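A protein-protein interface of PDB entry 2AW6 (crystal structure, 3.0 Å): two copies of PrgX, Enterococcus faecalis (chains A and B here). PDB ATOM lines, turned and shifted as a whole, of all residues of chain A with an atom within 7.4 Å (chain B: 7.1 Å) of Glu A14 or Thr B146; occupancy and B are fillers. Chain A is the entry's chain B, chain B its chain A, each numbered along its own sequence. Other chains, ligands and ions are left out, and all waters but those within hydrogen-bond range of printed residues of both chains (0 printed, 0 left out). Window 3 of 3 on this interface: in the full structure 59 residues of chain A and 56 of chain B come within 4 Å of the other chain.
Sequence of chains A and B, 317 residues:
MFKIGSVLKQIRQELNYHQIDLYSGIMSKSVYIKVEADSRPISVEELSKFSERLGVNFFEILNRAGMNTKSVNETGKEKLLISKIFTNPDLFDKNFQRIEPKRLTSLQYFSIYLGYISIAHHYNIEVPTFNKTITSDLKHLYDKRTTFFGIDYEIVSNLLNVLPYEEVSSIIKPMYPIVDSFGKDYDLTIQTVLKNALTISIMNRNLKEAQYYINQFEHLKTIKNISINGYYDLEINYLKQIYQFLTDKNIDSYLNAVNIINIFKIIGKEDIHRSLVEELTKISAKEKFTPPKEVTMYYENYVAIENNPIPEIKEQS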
ATOM      1  N   LEU A   8       9.678 -16.576   2.603  1.00  0.00           N
ATOM      2  CA  LEU A   8       9.801 -17.933   2.112  1.00  0.00           C
ATOM      3  C   LEU A   8       9.759 -17.906   0.591  1.00  0.00           C
ATOM      4  O   LEU A   8      10.638 -18.469  -0.066  1.00  0.00           O
ATOM      5  CB  LEU A   8       8.688 -18.805   2.673  1.00  0.00           C
ATOM      6  CG  LEU A   8       8.675 -19.060   4.180  1.00  0.00           C
ATOM      7  CD1 LEU A   8       7.273 -19.428   4.631  1.00  0.00           C
ATOM      8  CD2 LEU A   8       9.667 -20.151   4.561  1.00  0.00           C
ATOM      9  N   LYS A   9       8.756 -17.217   0.042  1.00  0.00           N
ATOM     10  CA  LYS A   9       8.631 -17.029  -1.408  1.00  0.00           C
ATOM     11  C   LYS A   9       9.892 -16.418  -2.004  1.00  0.00           C
ATOM     12  O   LYS A   9      10.402 -16.892  -3.019  1.00  0.00           O
ATOM     13  CB  LYS A   9       7.432 -16.134  -1.741  1.00  0.00           C
ATOM     14  CG  LYS A   9       7.109 -16.068  -3.235  1.00  0.00           C
ATOM     15  CD  LYS A   9       5.936 -15.145  -3.502  1.00  0.00           C
ATOM     16  CE  LYS A   9       5.704 -14.954  -4.990  1.00  0.00           C
ATOM     17  NZ  LYS A   9       4.673 -13.901  -5.199  1.00  0.00           N
ATOM     18  N   GLN A  10      10.377 -15.361  -1.353  1.00  0.00           N
ATOM     19  CA  GLN A  10      11.560 -14.638  -1.787  1.00  0.00           C
ATOM     20  C   GLN A  10      12.785 -15.555  -1.838  1.00  0.00           C
ATOM     21  O   GLN A  10      13.509 -15.577  -2.837  1.00  0.00           O
ATOM     22  CB  GLN A  10      11.804 -13.441  -0.872  1.00  0.00           C
ATOM     23  CG  GLN A  10      12.869 -12.486  -1.369  1.00  0.00           C
ATOM     24  CD  GLN A  10      13.648 -11.857  -0.234  1.00  0.00           C
ATOM     25  OE1 GLN A  10      14.876 -11.970  -0.175  1.00  0.00           O
ATOM     26  NE2 GLN A  10      12.936 -11.203   0.687  1.00  0.00           N
ATOM     27  N   ILE A  11      12.996 -16.324  -0.775  1.00  0.00           N
ATOM     28  CA  ILE A  11      14.127 -17.247  -0.716  1.00  0.00           C
ATOM     29  C   ILE A  11      13.957 -18.398  -1.707  1.00  0.00           C
ATOM     30  O   ILE A  11      14.907 -18.768  -2.407  1.00  0.00           O
ATOM     31  CB  ILE A  11      14.342 -17.790   0.716  1.00  0.00           C
ATOM     32  CG1 ILE A  11      14.755 -16.652   1.648  1.00  0.00           C
ATOM     33  CG2 ILE A  11      15.388 -18.897   0.726  1.00  0.00           C
ATOM     34  CD1 ILE A  11      14.601 -16.980   3.107  1.00  0.00           C
ATOM     35  N   ARG A  12      12.745 -18.945  -1.764  1.00  0.00           N
ATOM     36  CA  ARG A  12      12.423 -20.050  -2.658  1.00  0.00           C
ATOM     37  C   ARG A  12      12.832 -19.730  -4.089  1.00  0.00           C
ATOM     38  O   ARG A  12      13.586 -20.479  -4.719  1.00  0.00           O
ATOM     39  CB  ARG A  12      10.923 -20.336  -2.618  1.00  0.00           C
ATOM     40  CG  ARG A  12      10.596 -21.786  -2.841  1.00  0.00           C
ATOM     41  CD  ARG A  12       9.161 -21.972  -3.209  1.00  0.00           C
ATOM     42  NE  ARG A  12       8.932 -21.598  -4.597  1.00  0.00           N
ATOM     43  CZ  ARG A  12       8.175 -20.581  -4.983  1.00  0.00           C
ATOM     44  NH1 ARG A  12       7.554 -19.829  -4.086  1.00  0.00           N
ATOM     45  NH2 ARG A  12       8.029 -20.323  -6.275  1.00  0.00           N
ATOM     46  N   GLN A  13      12.330 -18.598  -4.580  1.00  0.00           N
ATOM     47  CA  GLN A  13      12.585 -18.123  -5.944  1.00  0.00           C
ATOM     48  C   GLN A  13      14.048 -17.781  -6.182  1.00  0.00           C
ATOM     49  O   GLN A  13      14.557 -17.963  -7.284  1.00  0.00           O
ATOM     50  CB  GLN A  13      11.723 -16.903  -6.262  1.00  0.00           C
ATOM     51  CG  GLN A  13      10.297 -17.229  -6.650  1.00  0.00           C
ATOM     52  CD  GLN A  13       9.397 -16.012  -6.599  1.00  0.00           C
ATOM     53  OE1 GLN A  13       8.283 -16.029  -7.121  1.00  0.00           O
ATOM     54  NE2 GLN A  13       9.877 -14.943  -5.965  1.00  0.00           N
ATOM     55  N   GLU A  14      14.716 -17.283  -5.148  1.00  0.00           N
ATOM     56  CA  GLU A  14      16.135 -16.961  -5.225  1.00  0.00           C
ATOM     57  C   GLU A  14      17.003 -18.229  -5.346  1.00  0.00           C
ATOM     58  O   GLU A  14      18.101 -18.179  -5.904  1.00  0.00           O
ATOM     59  CB  GLU A  14      16.535 -16.085  -4.020  1.00  0.00           C
ATOM     60  CG  GLU A  14      18.035 -15.848  -3.808  1.00  0.00           C
ATOM     61  CD  GLU A  14      18.707 -15.162  -4.977  1.00  0.00           C
ATOM     62  OE1 GLU A  14      19.955 -15.204  -5.053  1.00  0.00           O
ATOM     63  OE2 GLU A  14      17.993 -14.579  -5.816  1.00  0.00           O
ATOM     64  N   LEU A  15      16.497 -19.356  -4.847  1.00  0.00           N
ATOM     65  CA  LEU A  15      17.218 -20.626  -4.910  1.00  0.00           C
ATOM     66  C   LEU A  15      16.699 -21.523  -6.029  1.00  0.00           C
ATOM     67  O   LEU A  15      17.120 -22.673  -6.157  1.00  0.00           O
ATOM     68  CB  LEU A  15      17.134 -21.349  -3.562  1.00  0.00           C
ATOM     69  CG  LEU A  15      18.173 -21.106  -2.463  1.00  0.00           C
ATOM     70  CD1 LEU A  15      18.626 -19.666  -2.394  1.00  0.00           C
ATOM     71  CD2 LEU A  15      17.598 -21.527  -1.133  1.00  0.00           C
ATOM     72  N   ASN A  16      15.789 -20.979  -6.834  1.00  0.00           N
ATOM     73  CA  ASN A  16      15.141 -21.695  -7.937  1.00  0.00           C
ATOM     74  C   ASN A  16      14.476 -23.019  -7.540  1.00  0.00           C
ATOM     75  O   ASN A  16      14.469 -23.977  -8.318  1.00  0.00           O
ATOM     76  CB  ASN A  16      16.102 -21.870  -9.123  1.00  0.00           C
ATOM     77  CG  ASN A  16      16.488 -20.542  -9.768  1.00  0.00           C
ATOM     78  OD1 ASN A  16      15.634 -19.698 -10.060  1.00  0.00           O
ATOM     79  ND2 ASN A  16      17.784 -20.357 -10.000  1.00  0.00           N
ATOM     80  N   TYR A  17      13.925 -23.063  -6.324  1.00  0.00           N
ATOM     81  CA  TYR A  17      13.079 -24.176  -5.888  1.00  0.00           C
ATOM     82  C   TYR A  17      11.631 -23.922  -6.302  1.00  0.00           C
ATOM     83  O   TYR A  17      11.178 -22.773  -6.349  1.00  0.00           O
ATOM     84  CB  TYR A  17      13.158 -24.393  -4.373  1.00  0.00           C
ATOM     85  CG  TYR A  17      14.523 -24.779  -3.824  1.00  0.00           C
ATOM     86  CD1 TYR A  17      15.464 -25.466  -4.599  1.00  0.00           C
ATOM     87  CD2 TYR A  17      14.858 -24.481  -2.501  1.00  0.00           C
ATOM     88  CE1 TYR A  17      16.725 -25.821  -4.069  1.00  0.00           C
ATOM     89  CE2 TYR A  17      16.095 -24.834  -1.959  1.00  0.00           C
ATOM     90  CZ  TYR A  17      17.025 -25.499  -2.739  1.00  0.00           C
ATOM     91  OH  TYR A  17      18.247 -25.826  -2.178  1.00  0.00           O
ATOM     92  N   LEU B 141      25.824 -23.231  -8.432  1.00  0.00           N
ATOM     93  CA  LEU B 141      25.214 -22.619  -7.261  1.00  0.00           C
ATOM     94  C   LEU B 141      25.104 -21.110  -7.328  1.00  0.00           C
ATOM     95  O   LEU B 141      24.191 -20.544  -6.732  1.00  0.00           O
ATOM     96  CB  LEU B 141      25.925 -23.050  -5.978  1.00  0.00           C
ATOM     97  CG  LEU B 141      25.693 -24.523  -5.620  1.00  0.00           C
ATOM     98  CD1 LEU B 141      26.565 -24.950  -4.445  1.00  0.00           C
ATOM     99  CD2 LEU B 141      24.209 -24.831  -5.354  1.00  0.00           C
ATOM    100  N   TYR B 142      26.005 -20.460  -8.063  1.00  0.00           N
ATOM    101  CA  TYR B 142      26.132 -18.998  -7.981  1.00  0.00           C
ATOM    102  C   TYR B 142      25.927 -18.152  -9.246  1.00  0.00           C
ATOM    103  O   TYR B 142      25.685 -16.951  -9.136  1.00  0.00           O
ATOM    104  CB  TYR B 142      27.442 -18.620  -7.281  1.00  0.00           C
ATOM    105  CG  TYR B 142      27.440 -18.967  -5.811  1.00  0.00           C
ATOM    106  CD1 TYR B 142      26.470 -18.443  -4.956  1.00  0.00           C
ATOM    107  CD2 TYR B 142      28.398 -19.818  -5.272  1.00  0.00           C
ATOM    108  CE1 TYR B 142      26.452 -18.762  -3.595  1.00  0.00           C
ATOM    109  CE2 TYR B 142      28.394 -20.138  -3.911  1.00  0.00           C
ATOM    110  CZ  TYR B 142      27.416 -19.605  -3.077  1.00  0.00           C
ATOM    111  OH  TYR B 142      27.395 -19.914  -1.735  1.00  0.00           O
ATOM    112  N   LYS B 144      23.615 -17.480 -11.108  1.00  0.00           N
ATOM    113  CA  LYS B 144      22.315 -16.834 -11.298  1.00  0.00           C
ATOM    114  C   LYS B 144      21.711 -16.267  -9.998  1.00  0.00           C
ATOM    115  O   LYS B 144      20.493 -16.093  -9.876  1.00  0.00           O
ATOM    116  CB  LYS B 144      21.355 -17.809 -12.001  1.00  0.00           C
ATOM    117  CG  LYS B 144      21.689 -18.087 -13.483  1.00  0.00           C
ATOM    118  CD  LYS B 144      20.764 -17.325 -14.430  1.00  0.00           C
ATOM    119  CE  LYS B 144      21.038 -15.816 -14.428  1.00  0.00           C
ATOM    120  NZ  LYS B 144      19.782 -14.989 -14.460  1.00  0.00           N
ATOM    121  N   ARG B 145      22.576 -15.958  -9.036  1.00  0.00           N
ATOM    122  CA  ARG B 145      22.138 -15.449  -7.735  1.00  0.00           C
ATOM    123  C   ARG B 145      22.015 -13.923  -7.717  1.00  0.00           C
ATOM    124  O   ARG B 145      22.654 -13.237  -8.507  1.00  0.00           O
ATOM    125  CB  ARG B 145      23.090 -15.918  -6.624  1.00  0.00           C
ATOM    126  CG  ARG B 145      23.139 -17.433  -6.393  1.00  0.00           C
ATOM    127  CD  ARG B 145      21.848 -18.013  -5.789  1.00  0.00           C
ATOM    128  NE  ARG B 145      21.524 -17.416  -4.493  1.00  0.00           N
ATOM    129  CZ  ARG B 145      22.104 -17.728  -3.333  1.00  0.00           C
ATOM    130  NH1 ARG B 145      23.060 -18.652  -3.271  1.00  0.00           N
ATOM    131  NH2 ARG B 145      21.730 -17.101  -2.221  1.00  0.00           N
ATOM    132  N   THR B 146      21.186 -13.403  -6.812  1.00  0.00           N
ATOM    133  CA  THR B 146      21.033 -11.952  -6.628  1.00  0.00           C
ATOM    134  C   THR B 146      21.231 -11.475  -5.187  1.00  0.00           C
ATOM    135  O   THR B 146      21.850 -10.446  -4.963  1.00  0.00           O
ATOM    136  CB  THR B 146      19.671 -11.421  -7.129  1.00  0.00           C
ATOM    137  OG1 THR B 146      18.598 -12.124  -6.483  1.00  0.00           O
ATOM    138  CG2 THR B 146      19.553 -11.558  -8.636  1.00  0.00           C
ATOM    139  N   THR B 147      20.678 -12.204  -4.223  1.00  0.00           N
ATOM    140  CA  THR B 147      20.879 -11.909  -2.794  1.00  0.00           C
ATOM    141  C   THR B 147      21.539 -13.069  -2.059  1.00  0.00           C
ATOM    142  O   THR B 147      21.387 -14.234  -2.448  1.00  0.00           O
ATOM    143  CB  THR B 147      19.557 -11.576  -2.053  1.00  0.00           C
ATOM    144  OG1 THR B 147      18.440 -11.947  -2.870  1.00  0.00           O
ATOM    145  CG2 THR B 147      19.474 -10.088  -1.720  1.00  0.00           C
ATOM    146  N   PHE B 148      22.243 -12.746  -0.978  1.00  0.00           N
ATOM    147  CA  PHE B 148      23.027 -13.748  -0.266  1.00  0.00           C
ATOM    148  C   PHE B 148      22.655 -13.918   1.201  1.00  0.00           C
ATOM    149  O   PHE B 148      22.422 -12.939   1.924  1.00  0.00           O
ATOM    150  CB  PHE B 148      24.518 -13.474  -0.463  1.00  0.00           C
ATOM    151  CG  PHE B 148      24.907 -13.421  -1.906  1.00  0.00           C
ATOM    152  CD1 PHE B 148      25.052 -12.197  -2.556  1.00  0.00           C
ATOM    153  CD2 PHE B 148      25.058 -14.592  -2.637  1.00  0.00           C
ATOM    154  CE1 PHE B 148      25.386 -12.133  -3.910  1.00  0.00           C
ATOM    155  CE2 PHE B 148      25.390 -14.545  -3.985  1.00  0.00           C
ATOM    156  CZ  PHE B 148      25.553 -13.310  -4.623  1.00  0.00           C
ATOM    157  N   PHE B 149      22.598 -15.178   1.625  1.00  0.00           N
ATOM    158  CA  PHE B 149      22.150 -15.534   2.961  1.00  0.00           C
ATOM    159  C   PHE B 149      23.315 -15.968   3.824  1.00  0.00           C
ATOM    160  O   PHE B 149      24.408 -16.215   3.317  1.00  0.00           O
ATOM    161  CB  PHE B 149      21.093 -16.628   2.884  1.00  0.00           C
ATOM    162  CG  PHE B 149      20.002 -16.333   1.895  1.00  0.00           C
ATOM    163  CD1 PHE B 149      19.959 -16.998   0.667  1.00  0.00           C
ATOM    164  CD2 PHE B 149      19.024 -15.368   2.178  1.00  0.00           C
ATOM    165  CE1 PHE B 149      18.960 -16.719  -0.263  1.00  0.00           C
ATOM    166  CE2 PHE B 149      18.013 -15.072   1.254  1.00  0.00           C
ATOM    167  CZ  PHE B 149      17.983 -15.750   0.027  1.00  0.00           C
ATOM    168  N   ASP B 152      25.494 -18.711   2.631  1.00  0.00           N
ATOM    169  CA  ASP B 152      26.337 -18.332   1.497  1.00  0.00           C
ATOM    170  C   ASP B 152      27.668 -17.788   1.987  1.00  0.00           C
ATOM    171  O   ASP B 152      28.726 -18.247   1.542  1.00  0.00           O
ATOM    172  CB  ASP B 152      25.640 -17.300   0.617  1.00  0.00           C
ATOM    173  CG  ASP B 152      24.445 -17.868  -0.112  1.00  0.00           C
ATOM    174  OD1 ASP B 152      23.335 -17.331   0.072  1.00  0.00           O
ATOM    175  OD2 ASP B 152      24.612 -18.849  -0.867  1.00  0.00           O
ATOM    176  N   PRO B 174      30.443  -9.594  -5.359  1.00  0.00           N
ATOM    177  CA  PRO B 174      29.010  -9.286  -5.385  1.00  0.00           C
ATOM    178  C   PRO B 174      28.310  -9.361  -4.033  1.00  0.00           C
ATOM    179  O   PRO B 174      27.230  -8.798  -3.880  1.00  0.00           O
ATOM    180  CB  PRO B 174      28.425 -10.356  -6.325  1.00  0.00           C
ATOM    181  CG  PRO B 174      29.585 -10.910  -7.059  1.00  0.00           C
ATOM    182  CD  PRO B 174      30.737 -10.822  -6.110  1.00  0.00           C
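The side-chain carboxylate (OE1) of Glu A14 is in salt-bridge range of the guanidinium group (NE) of Arg B145 (2.8 Å). The side-chain carboxylate of Glu A14 is in hydrogen-bond range of the side-chain hydroxyl of Thr B146, 2.6 Å away. The backbone NH (N) of Thr B147 is in hydrogen-bond range of the side-chain carboxylate (OE1) of Glu A14, 3.2 Å away.
The guanidinium group (NH2) of Arg B145 lies within salt-bridge range of the side-chain carboxylate (OD1) of Asp B152 (2.8 Å). The guanidinium group (NH2) of Arg B145 sits at hydrogen-bond distance from the backbone carbonyl oxygen (O) of Thr B147, 2.9 Å away. The backbone NH (N) of Phe B149 is in hydrogen-bond range of the side-chain carboxylate (OD1) of Asp B152 (2.8 Å).
Phe B149 touches Ile A11. CG of Glu A14 touches CE1 of Phe B149, at 3.8 Å. CE1 of Phe B149 touches CD1 of Leu A15, 3.7 Å away.
Leu A8 touches none of the printed residues of chain B. Printed residues of chain B within 4 Å of Ile A11: Phe B149 (3.6 Å). Glu A14 touches just these residues of chain B: Arg B145, Thr B146, Thr B147 and Phe B149. Of the printed residues of chain B, Leu A15 touches Phe B149. Tyr B142 touches none of the printed residues of chain A. Of the printed residues of chain A, Arg B145 touches Glu A14 (2.8 Å). Of chain A, only Glu A14 (2.6 Å) comes within 4 Å of Thr B146. Of the printed residues of chain A, Phe B149 touches Ile A11, Glu A14 and Leu A15. The nearest printed residue of chain A that does not touch Thr B146 is Gln A13 (7.1 Å). The nearest printed residue of chain B that does not touch Ile A11 is Arg B145 (7.0 Å).
Of the 10 printed residues of chain A, 3 touch a printed residue of chain B. Hydrophobic or aromatic side chains of chain A within 4 Å of the printed part of chain B: Ile A11 and Leu A15. Along chain A the printed residues that touch a printed residue of chain B span positions 11 to 15. Printed residues of chain B that touch a printed residue of chain A: Arg B145, Thr B146, Thr B147 and Phe B149. Hydrophobic or aromatic side chains of chain B within 4 Å of the printed part of chain A: Phe B149. Along chain B the printed residues that touch a printed residue of chain A span positions 145 to 149. Among the printed residues, 6 pairs touch across the chains.
No position is printed for both chains.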
